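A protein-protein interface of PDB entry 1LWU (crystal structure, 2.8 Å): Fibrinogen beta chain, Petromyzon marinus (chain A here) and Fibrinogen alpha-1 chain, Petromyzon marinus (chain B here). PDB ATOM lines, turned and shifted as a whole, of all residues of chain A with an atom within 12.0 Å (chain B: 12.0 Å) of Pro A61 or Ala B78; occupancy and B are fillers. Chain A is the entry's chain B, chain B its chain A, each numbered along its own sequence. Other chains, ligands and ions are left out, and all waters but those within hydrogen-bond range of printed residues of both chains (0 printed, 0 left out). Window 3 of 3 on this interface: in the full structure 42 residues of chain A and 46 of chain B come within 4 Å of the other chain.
Of chain B, only Ser B76 (3.5 Å), Cys B77 (3.9 Å) and Ala B78 (3.4 Å) come within 4 Å of Pro A61.
Ala B78 touches just these residues of chain A: Leu A57, Ala A60, Pro A61 and Cys A62.
Of chain B, only Cys B77, Ala B78, Arg B79 and Leu B81 come within 4 Å of Leu A57.
Cys A58 touches just one residue of chain B: Cys B77 (2.0 Å).
Of chain B, only Cys B77 and Ala B78 come within 4 Å of Ala A60.
No residue of chain B comes within 4 Å of Thr A63.
Ser B76 touches just these residues of chain A: Pro A61 and Cys A62.
Cys B77 touches just these residues of chain A: Leu A57, Cys A58, Ala A60, Pro A61 and Cys A62.
Of the printed residues of chain A, Tyr B80 touches Gln A54 (3.2 Å).
Printed residues of chain B within 4 Å of Gln A54: Cys B73, Arg B79, Tyr B80 and Leu B81.
Of the printed residues of chain A, Cys B73 touches Gln A54 (3.3 Å).
Printed residues of chain B within 4 Å of Asn A140: Gly B75.
Gln A54 touches Arg B79 (NE2 to O, 3.7 Å).
Tyr B80 touches Gln A54.
O of Leu A57 touches CB of Cys B77, at 3.3 Å.
Ala B78 touches Leu A57.
Leu A57 touches Leu B81 (CD1 to CD2, 3.3 Å).
Ala A60 touches Cys B77 (O to CA, 3.8 Å).
Ser B76 touches Pro A61 (O to CA, 3.5 Å).
Cys B77 touches Pro A61 (C to C, 3.9 Å).
Cys A62 touches Cys B77.
Ser A124 touches Arg B71.
The backbone carbonyl oxygen (O) of Ala B72 sits close to the backbone carbonyl oxygen (O) of Ser A124.
O of Ser A124 sits at hydrogen-bond distance from N of Gly B75, 3.3 Å away.
The side-chain amide nitrogen (ND2) of Asn A140 sits at hydrogen-bond distance from the backbone carbonyl oxygen (O) of Gly B75, at 2.7 Å.
N of Cys A62 is in hydrogen-bond range of O of Ser B76.
The side-chain sulfur (SG) of Cys B77 forms a disulfide with the side-chain sulfur (SG) of Cys A58 (2.0 Å).
N of Ala B78 lies within hydrogen-bond range of O of Ala A60 (2.9 Å).
The backbone NH (N) of Ala B78 lies close to the backbone carbonyl oxygen (O) of Pro A61 (3.5 Å).
The side-chain amide nitrogen of Gln A54 lies close to the backbone NH of Leu B81 (2.8 Å).
The backbone carbonyl oxygen of Arg B79 sits close to the backbone carbonyl oxygen of Leu A57.
The side-chain sulfur (SG) of Cys A62 lies close to the backbone carbonyl oxygen (O) of Gly B75 (3.2 Å).
Of the 18 printed residues of chain A, 9 touch a printed residue of chain B.
Printed residues of chain A that touch a printed residue of chain B: Gln A54, Leu A57, Cys A58, Ala A60, Pro A61, Cys A62, Ser A124, Asn A140 and Phe A143.
Of the 13 printed residues of chain B, 10 touch a printed residue of chain A.
Among the printed residues, 23 pairs touch across the chains.
OE1 of Glu B82 lies within salt-bridge range of NH2 of Arg B71 (3.2 Å).
OH of Tyr B80 lies within hydrogen-bond range of OE2 of Glu B82 (3.2 Å).
The side-chain sulfur (SG) of Cys A58 sits close to the side-chain amide oxygen (OE1) of Gln A54, 3.6 Å away.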
ATOM      1  N   THR A  53      11.994  30.949 -14.938  1.00  0.00           N
ATOM      2  CA  THR A  53      11.464  31.001 -13.574  1.00  0.00           C
ATOM      3  C   THR A  53      12.464  30.442 -12.546  1.00  0.00           C
ATOM      4  O   THR A  53      12.721  31.073 -11.516  1.00  0.00           O
ATOM      5  CB  THR A  53      10.113  30.234 -13.467  1.00  0.00           C
ATOM      6  OG1 THR A  53       9.076  31.032 -14.047  1.00  0.00           O
ATOM      7  CG2 THR A  53       9.753  29.941 -12.018  1.00  0.00           C
ATOM      8  N   GLN A  54      13.029  29.268 -12.818  1.00  0.00           N
ATOM      9  CA  GLN A  54      13.994  28.693 -11.890  1.00  0.00           C
ATOM     10  C   GLN A  54      15.255  29.534 -11.834  1.00  0.00           C
ATOM     11  O   GLN A  54      15.799  29.743 -10.758  1.00  0.00           O
ATOM     12  CB  GLN A  54      14.364  27.258 -12.283  1.00  0.00           C
ATOM     13  CG  GLN A  54      13.720  26.182 -11.415  1.00  0.00           C
ATOM     14  CD  GLN A  54      13.875  26.470  -9.937  1.00  0.00           C
ATOM     15  OE1 GLN A  54      14.939  26.891  -9.483  1.00  0.00           O
ATOM     16  NE2 GLN A  54      12.811  26.239  -9.176  1.00  0.00           N
ATOM     17  N   LYS A  55      15.724  30.012 -12.986  1.00  0.00           N
ATOM     18  CA  LYS A  55      16.927  30.835 -13.001  1.00  0.00           C
ATOM     19  C   LYS A  55      16.720  32.024 -12.067  1.00  0.00           C
ATOM     20  O   LYS A  55      17.574  32.334 -11.230  1.00  0.00           O
ATOM     21  CB  LYS A  55      17.229  31.341 -14.408  1.00  0.00           C
ATOM     22  CG  LYS A  55      18.551  32.097 -14.493  1.00  0.00           C
ATOM     23  CD  LYS A  55      18.767  32.700 -15.877  1.00  0.00           C
ATOM     24  CE  LYS A  55      20.132  33.381 -16.001  1.00  0.00           C
ATOM     25  NZ  LYS A  55      21.293  32.438 -15.949  1.00  0.00           N
ATOM     26  N   GLU A  56      15.571  32.677 -12.208  1.00  0.00           N
ATOM     27  CA  GLU A  56      15.226  33.822 -11.367  1.00  0.00           C
ATOM     28  C   GLU A  56      15.267  33.458  -9.886  1.00  0.00           C
ATOM     29  O   GLU A  56      15.835  34.184  -9.082  1.00  0.00           O
ATOM     30  CB  GLU A  56      13.829  34.346 -11.726  1.00  0.00           C
ATOM     31  CG  GLU A  56      13.372  35.573 -10.932  1.00  0.00           C
ATOM     32  CD  GLU A  56      14.299  36.776 -11.100  1.00  0.00           C
ATOM     33  OE1 GLU A  56      14.661  37.091 -12.261  1.00  0.00           O
ATOM     34  OE2 GLU A  56      14.655  37.410 -10.074  1.00  0.00           O
ATOM     35  N   LEU A  57      14.671  32.331  -9.534  1.00  0.00           N
ATOM     36  CA  LEU A  57      14.654  31.866  -8.147  1.00  0.00           C
ATOM     37  C   LEU A  57      15.977  31.281  -7.642  1.00  0.00           C
ATOM     38  O   LEU A  57      15.980  30.678  -6.560  1.00  0.00           O
ATOM     39  CB  LEU A  57      13.561  30.820  -7.967  1.00  0.00           C
ATOM     40  CG  LEU A  57      12.152  31.253  -8.371  1.00  0.00           C
ATOM     41  CD1 LEU A  57      11.245  30.035  -8.461  1.00  0.00           C
ATOM     42  CD2 LEU A  57      11.622  32.254  -7.367  1.00  0.00           C
ATOM     43  N   CYS A  58      17.065  31.434  -8.429  1.00  0.00           N
ATOM     44  CA  CYS A  58      18.410  30.955  -8.051  1.00  0.00           C
ATOM     45  C   CYS A  58      19.346  32.131  -7.858  1.00  0.00           C
ATOM     46  O   CYS A  58      20.572  31.970  -7.804  1.00  0.00           O
ATOM     47  CB  CYS A  58      19.020  30.016  -9.102  1.00  0.00           C
ATOM     48  SG  CYS A  58      18.175  28.407  -9.208  1.00  0.00           S
ATOM     49  N   SER A  59      18.758  33.321  -7.774  1.00  0.00           N
ATOM     50  CA  SER A  59      19.522  34.537  -7.552  1.00  0.00           C
ATOM     51  C   SER A  59      20.227  34.326  -6.214  1.00  0.00           C
ATOM     52  O   SER A  59      21.381  34.722  -6.022  1.00  0.00           O
ATOM     53  CB  SER A  59      18.575  35.739  -7.479  1.00  0.00           C
ATOM     54  OG  SER A  59      19.301  36.958  -7.454  1.00  0.00           O
ATOM     55  N   ALA A  60      19.512  33.677  -5.299  1.00  0.00           N
ATOM     56  CA  ALA A  60      20.029  33.365  -3.976  1.00  0.00           C
ATOM     57  C   ALA A  60      20.084  31.844  -3.809  1.00  0.00           C
ATOM     58  O   ALA A  60      19.148  31.140  -4.169  1.00  0.00           O
ATOM     59  CB  ALA A  60      19.131  33.969  -2.922  1.00  0.00           C
ATOM     60  N   PRO A  61      21.186  31.316  -3.261  1.00  0.00           N
ATOM     61  CA  PRO A  61      21.297  29.868  -3.073  1.00  0.00           C
ATOM     62  C   PRO A  61      20.365  29.448  -1.953  1.00  0.00           C
ATOM     63  O   PRO A  61      19.736  30.290  -1.320  1.00  0.00           O
ATOM     64  CB  PRO A  61      22.749  29.692  -2.666  1.00  0.00           C
ATOM     65  CG  PRO A  61      22.954  30.901  -1.790  1.00  0.00           C
ATOM     66  CD  PRO A  61      22.331  32.010  -2.642  1.00  0.00           C
ATOM     67  N   CYS A  62      20.271  28.148  -1.707  1.00  0.00           N
ATOM     68  CA  CYS A  62      19.437  27.675  -0.622  1.00  0.00           C
ATOM     69  C   CYS A  62      20.338  27.547   0.579  1.00  0.00           C
ATOM     70  O   CYS A  62      21.558  27.613   0.452  1.00  0.00           O
ATOM     71  CB  CYS A  62      18.805  26.324  -0.945  1.00  0.00           C
ATOM     72  SG  CYS A  62      19.948  25.037  -1.513  1.00  0.00           S
ATOM     73  N   THR A  63      19.731  27.361   1.743  1.00  0.00           N
ATOM     74  CA  THR A  63      20.478  27.241   2.978  1.00  0.00           C
ATOM     75  C   THR A  63      19.748  26.383   3.987  1.00  0.00           C
ATOM     76  O   THR A  63      18.517  26.366   4.039  1.00  0.00           O
ATOM     77  CB  THR A  63      20.678  28.614   3.631  1.00  0.00           C
ATOM     78  OG1 THR A  63      19.397  29.224   3.846  1.00  0.00           O
ATOM     79  CG2 THR A  63      21.536  29.517   2.746  1.00  0.00           C
ATOM     80  N   VAL A  64      20.521  25.666   4.787  1.00  0.00           N
ATOM     81  CA  VAL A  64      19.968  24.847   5.846  1.00  0.00           C
ATOM     82  C   VAL A  64      20.502  25.470   7.127  1.00  0.00           C
ATOM     83  O   VAL A  64      21.722  25.553   7.336  1.00  0.00           O
ATOM     84  CB  VAL A  64      20.412  23.378   5.738  1.00  0.00           C
ATOM     85  CG1 VAL A  64      19.638  22.692   4.634  1.00  0.00           C
ATOM     86  CG2 VAL A  64      21.900  23.299   5.473  1.00  0.00           C
ATOM     87  N   ASN A  65      19.580  25.927   7.969  1.00  0.00           N
ATOM     88  CA  ASN A  65      19.939  26.588   9.215  1.00  0.00           C
ATOM     89  C   ASN A  65      19.640  25.683  10.387  1.00  0.00           C
ATOM     90  O   ASN A  65      19.658  26.129  11.534  1.00  0.00           O
ATOM     91  CB  ASN A  65      19.141  27.888   9.346  1.00  0.00           C
ATOM     92  CG  ASN A  65      19.129  28.703   8.054  1.00  0.00           C
ATOM     93  OD1 ASN A  65      20.119  29.347   7.694  1.00  0.00           O
ATOM     94  ND2 ASN A  65      18.005  28.662   7.341  1.00  0.00           N
ATOM     95  N   SER A 124      17.148  16.459  -6.381  1.00  0.00           N
ATOM     96  CA  SER A 124      17.601  17.714  -5.799  1.00  0.00           C
ATOM     97  C   SER A 124      19.103  17.967  -5.920  1.00  0.00           C
ATOM     98  O   SER A 124      19.578  19.059  -5.607  1.00  0.00           O
ATOM     99  CB  SER A 124      17.182  17.793  -4.335  1.00  0.00           C
ATOM    100  OG  SER A 124      17.954  16.919  -3.550  1.00  0.00           O
ATOM    101  N   GLY A 139      26.369  17.402  -2.547  1.00  0.00           N
ATOM    102  CA  GLY A 139      24.956  17.294  -2.252  1.00  0.00           C
ATOM    103  C   GLY A 139      24.576  17.828  -0.885  1.00  0.00           C
ATOM    104  O   GLY A 139      25.394  18.417  -0.190  1.00  0.00           O
ATOM    105  N   ASN A 140      23.324  17.607  -0.504  1.00  0.00           N
ATOM    106  CA  ASN A 140      22.810  18.059   0.774  1.00  0.00           C
ATOM    107  C   ASN A 140      22.519  16.868   1.654  1.00  0.00           C
ATOM    108  O   ASN A 140      21.820  15.947   1.241  1.00  0.00           O
ATOM    109  CB  ASN A 140      21.522  18.850   0.568  1.00  0.00           C
ATOM    110  CG  ASN A 140      21.754  20.161  -0.134  1.00  0.00           C
ATOM    111  OD1 ASN A 140      22.527  21.012   0.333  1.00  0.00           O
ATOM    112  ND2 ASN A 140      21.081  20.343  -1.263  1.00  0.00           N
ATOM    113  N   PHE A 143      17.550  18.471   4.923  1.00  0.00           N
ATOM    114  CA  PHE A 143      16.879  19.769   4.888  1.00  0.00           C
ATOM    115  C   PHE A 143      16.112  20.003   6.186  1.00  0.00           C
ATOM    116  O   PHE A 143      15.809  19.040   6.901  1.00  0.00           O
ATOM    117  CB  PHE A 143      15.917  19.807   3.724  1.00  0.00           C
ATOM    118  CG  PHE A 143      16.577  19.715   2.384  1.00  0.00           C
ATOM    119  CD1 PHE A 143      17.357  20.762   1.902  1.00  0.00           C
ATOM    120  CD2 PHE A 143      16.372  18.610   1.574  1.00  0.00           C
ATOM    121  CE1 PHE A 143      17.920  20.711   0.627  1.00  0.00           C
ATOM    122  CE2 PHE A 143      16.929  18.550   0.297  1.00  0.00           C
ATOM    123  CZ  PHE A 143      17.706  19.606  -0.176  1.00  0.00           C
ATOM    124  N   GLY A 144      15.811  21.275   6.483  1.00  0.00           N
ATOM    125  CA  GLY A 144      15.086  21.648   7.699  1.00  0.00           C
ATOM    126  C   GLY A 144      13.663  21.118   7.712  1.00  0.00           C
ATOM    127  O   GLY A 144      12.899  21.352   6.775  1.00  0.00           O
ATOM    128  N   LEU B  70      16.275  21.051 -13.938  1.00  0.00           N
ATOM    129  CA  LEU B  70      15.446  21.903 -13.099  1.00  0.00           C
ATOM    130  C   LEU B  70      15.185  21.297 -11.719  1.00  0.00           C
ATOM    131  O   LEU B  70      15.178  21.999 -10.703  1.00  0.00           O
ATOM    132  CB  LEU B  70      14.113  22.147 -13.773  1.00  0.00           C
ATOM    133  CG  LEU B  70      13.942  23.505 -14.431  1.00  0.00           C
ATOM    134  CD1 LEU B  70      15.306  24.048 -14.830  1.00  0.00           C
ATOM    135  CD2 LEU B  70      13.012  23.353 -15.644  1.00  0.00           C
ATOM    136  N   ARG B  71      14.958  19.993 -11.681  1.00  0.00           N
ATOM    137  CA  ARG B  71      14.690  19.331 -10.425  1.00  0.00           C
ATOM    138  C   ARG B  71      15.900  19.466  -9.515  1.00  0.00           C
ATOM    139  O   ARG B  71      15.769  19.500  -8.291  1.00  0.00           O
ATOM    140  CB  ARG B  71      14.356  17.870 -10.708  1.00  0.00           C
ATOM    141  CG  ARG B  71      13.925  17.064  -9.513  1.00  0.00           C
ATOM    142  CD  ARG B  71      13.112  15.859  -9.955  1.00  0.00           C
ATOM    143  NE  ARG B  71      11.729  16.223 -10.263  1.00  0.00           N
ATOM    144  CZ  ARG B  71      11.196  16.245 -11.484  1.00  0.00           C
ATOM    145  NH1 ARG B  71      11.918  15.921 -12.547  1.00  0.00           N
ATOM    146  NH2 ARG B  71       9.924  16.591 -11.638  1.00  0.00           N
ATOM    147  N   ALA B  72      17.081  19.568 -10.126  1.00  0.00           N
ATOM    148  CA  ALA B  72      18.342  19.693  -9.386  1.00  0.00           C
ATOM    149  C   ALA B  72      18.345  20.943  -8.510  1.00  0.00           C
ATOM    150  O   ALA B  72      18.897  20.932  -7.408  1.00  0.00           O
ATOM    151  CB  ALA B  72      19.542  19.715 -10.367  1.00  0.00           C
ATOM    152  N   CYS B  73      17.696  22.003  -8.995  1.00  0.00           N
ATOM    153  CA  CYS B  73      17.638  23.269  -8.283  1.00  0.00           C
ATOM    154  C   CYS B  73      16.984  23.250  -6.922  1.00  0.00           C
ATOM    155  O   CYS B  73      17.219  24.144  -6.116  1.00  0.00           O
ATOM    156  CB  CYS B  73      16.943  24.299  -9.117  1.00  0.00           C
ATOM    157  SG  CYS B  73      17.612  24.367 -10.782  1.00  0.00           S
ATOM    158  N   LYS B  74      16.148  22.259  -6.661  1.00  0.00           N
ATOM    159  CA  LYS B  74      15.508  22.180  -5.359  1.00  0.00           C
ATOM    160  C   LYS B  74      16.604  22.250  -4.295  1.00  0.00           C
ATOM    161  O   LYS B  74      16.562  23.075  -3.383  1.00  0.00           O
ATOM    162  CB  LYS B  74      14.738  20.869  -5.245  1.00  0.00           C
ATOM    163  CG  LYS B  74      14.036  20.577  -3.913  1.00  0.00           C
ATOM    164  CD  LYS B  74      12.926  19.530  -4.184  1.00  0.00           C
ATOM    165  CE  LYS B  74      12.243  19.005  -2.922  1.00  0.00           C
ATOM    166  NZ  LYS B  74      13.037  17.970  -2.190  1.00  0.00           N
ATOM    167  N   GLY B  75      17.606  21.393  -4.428  1.00  0.00           N
ATOM    168  CA  GLY B  75      18.676  21.389  -3.447  1.00  0.00           C
ATOM    169  C   GLY B  75      19.757  22.419  -3.703  1.00  0.00           C
ATOM    170  O   GLY B  75      20.803  22.369  -3.050  1.00  0.00           O
ATOM    171  N   SER B  76      19.516  23.351  -4.632  1.00  0.00           N
ATOM    172  CA  SER B  76      20.501  24.386  -4.947  1.00  0.00           C
ATOM    173  C   SER B  76      20.058  25.850  -4.785  1.00  0.00           C
ATOM    174  O   SER B  76      20.864  26.710  -4.449  1.00  0.00           O
ATOM    175  CB  SER B  76      21.002  24.180  -6.364  1.00  0.00           C
ATOM    176  OG  SER B  76      21.901  25.202  -6.736  1.00  0.00           O
ATOM    177  N   CYS B  77      18.777  26.124  -5.016  1.00  0.00           N
ATOM    178  CA  CYS B  77      18.242  27.481  -4.929  1.00  0.00           C
ATOM    179  C   CYS B  77      17.296  27.780  -3.756  1.00  0.00           C
ATOM    180  O   CYS B  77      16.639  26.891  -3.206  1.00  0.00           O
ATOM    181  CB  CYS B  77      17.575  27.811  -6.261  1.00  0.00           C
ATOM    182  SG  CYS B  77      18.724  27.346  -7.576  1.00  0.00           S
ATOM    183  N   ALA B  78      17.247  29.056  -3.384  1.00  0.00           N
ATOM    184  CA  ALA B  78      16.418  29.530  -2.283  1.00  0.00           C
ATOM    185  C   ALA B  78      14.951  29.151  -2.476  1.00  0.00           C
ATOM    186  O   ALA B  78      14.286  28.710  -1.537  1.00  0.00           O
ATOM    187  CB  ALA B  78      16.565  31.046  -2.146  1.00  0.00           C
ATOM    188  N   ARG B  79      14.446  29.332  -3.691  1.00  0.00           N
ATOM    189  CA  ARG B  79      13.065  28.985  -3.990  1.00  0.00           C
ATOM    190  C   ARG B  79      13.048  27.979  -5.118  1.00  0.00           C
ATOM    191  O   ARG B  79      13.807  28.097  -6.084  1.00  0.00           O
ATOM    192  CB  ARG B  79      12.257  30.235  -4.375  1.00  0.00           C
ATOM    193  CG  ARG B  79      11.637  30.943  -3.182  1.00  0.00           C
ATOM    194  CD  ARG B  79      11.548  32.452  -3.370  1.00  0.00           C
ATOM    195  NE  ARG B  79      10.649  32.886  -4.443  1.00  0.00           N
ATOM    196  CZ  ARG B  79       9.383  32.506  -4.571  1.00  0.00           C
ATOM    197  NH1 ARG B  79       8.851  31.664  -3.697  1.00  0.00           N
ATOM    198  NH2 ARG B  79       8.648  32.994  -5.555  1.00  0.00           N
ATOM    199  N   TYR B  80      12.189  26.976  -4.981  1.00  0.00           N
ATOM    200  CA  TYR B  80      12.065  25.927  -5.988  1.00  0.00           C
ATOM    201  C   TYR B  80      10.629  25.755  -6.431  1.00  0.00           C
ATOM    202  O   TYR B  80       9.736  25.595  -5.604  1.00  0.00           O
ATOM    203  CB  TYR B  80      12.557  24.584  -5.442  1.00  0.00           C
ATOM    204  CG  TYR B  80      12.317  23.437  -6.401  1.00  0.00           C
ATOM    205  CD1 TYR B  80      12.940  23.412  -7.650  1.00  0.00           C
ATOM    206  CD2 TYR B  80      11.447  22.399  -6.079  1.00  0.00           C
ATOM    207  CE1 TYR B  80      12.705  22.396  -8.553  1.00  0.00           C
ATOM    208  CE2 TYR B  80      11.206  21.374  -6.981  1.00  0.00           C
ATOM    209  CZ  TYR B  80      11.840  21.380  -8.219  1.00  0.00           C
ATOM    210  OH  TYR B  80      11.607  20.377  -9.136  1.00  0.00           O
ATOM    211  N   LEU B  81      10.400  25.768  -7.735  1.00  0.00           N
ATOM    212  CA  LEU B  81       9.047  25.590  -8.221  1.00  0.00           C
ATOM    213  C   LEU B  81       8.720  24.129  -8.542  1.00  0.00           C
ATOM    214  O   LEU B  81       8.279  23.396  -7.662  1.00  0.00           O
ATOM    215  CB  LEU B  81       8.803  26.482  -9.438  1.00  0.00           C
ATOM    216  CG  LEU B  81       7.948  27.717  -9.145  1.00  0.00           C
ATOM    217  CD1 LEU B  81       6.506  27.311  -8.932  1.00  0.00           C
ATOM    218  CD2 LEU B  81       8.477  28.414  -7.918  1.00  0.00           C
ATOM    219  N   GLU B  82       8.938  23.707  -9.786  1.00  0.00           N
ATOM    220  CA  GLU B  82       8.626  22.340 -10.221  1.00  0.00           C
ATOM    221  C   GLU B  82       8.111  22.398 -11.653  1.00  0.00           C
ATOM    222  O   GLU B  82       7.061  22.978 -11.915  1.00  0.00           O
ATOM    223  CB  GLU B  82       7.532  21.707  -9.335  1.00  0.00           C
ATOM    224  CG  GLU B  82       6.921  20.404  -9.857  1.00  0.00           C
ATOM    225  CD  GLU B  82       7.756  19.172  -9.534  1.00  0.00           C
ATOM    226  OE1 GLU B  82       7.492  18.095 -10.120  1.00  0.00           O
ATOM    227  OE2 GLU B  82       8.672  19.274  -8.689  1.00  0.00           O
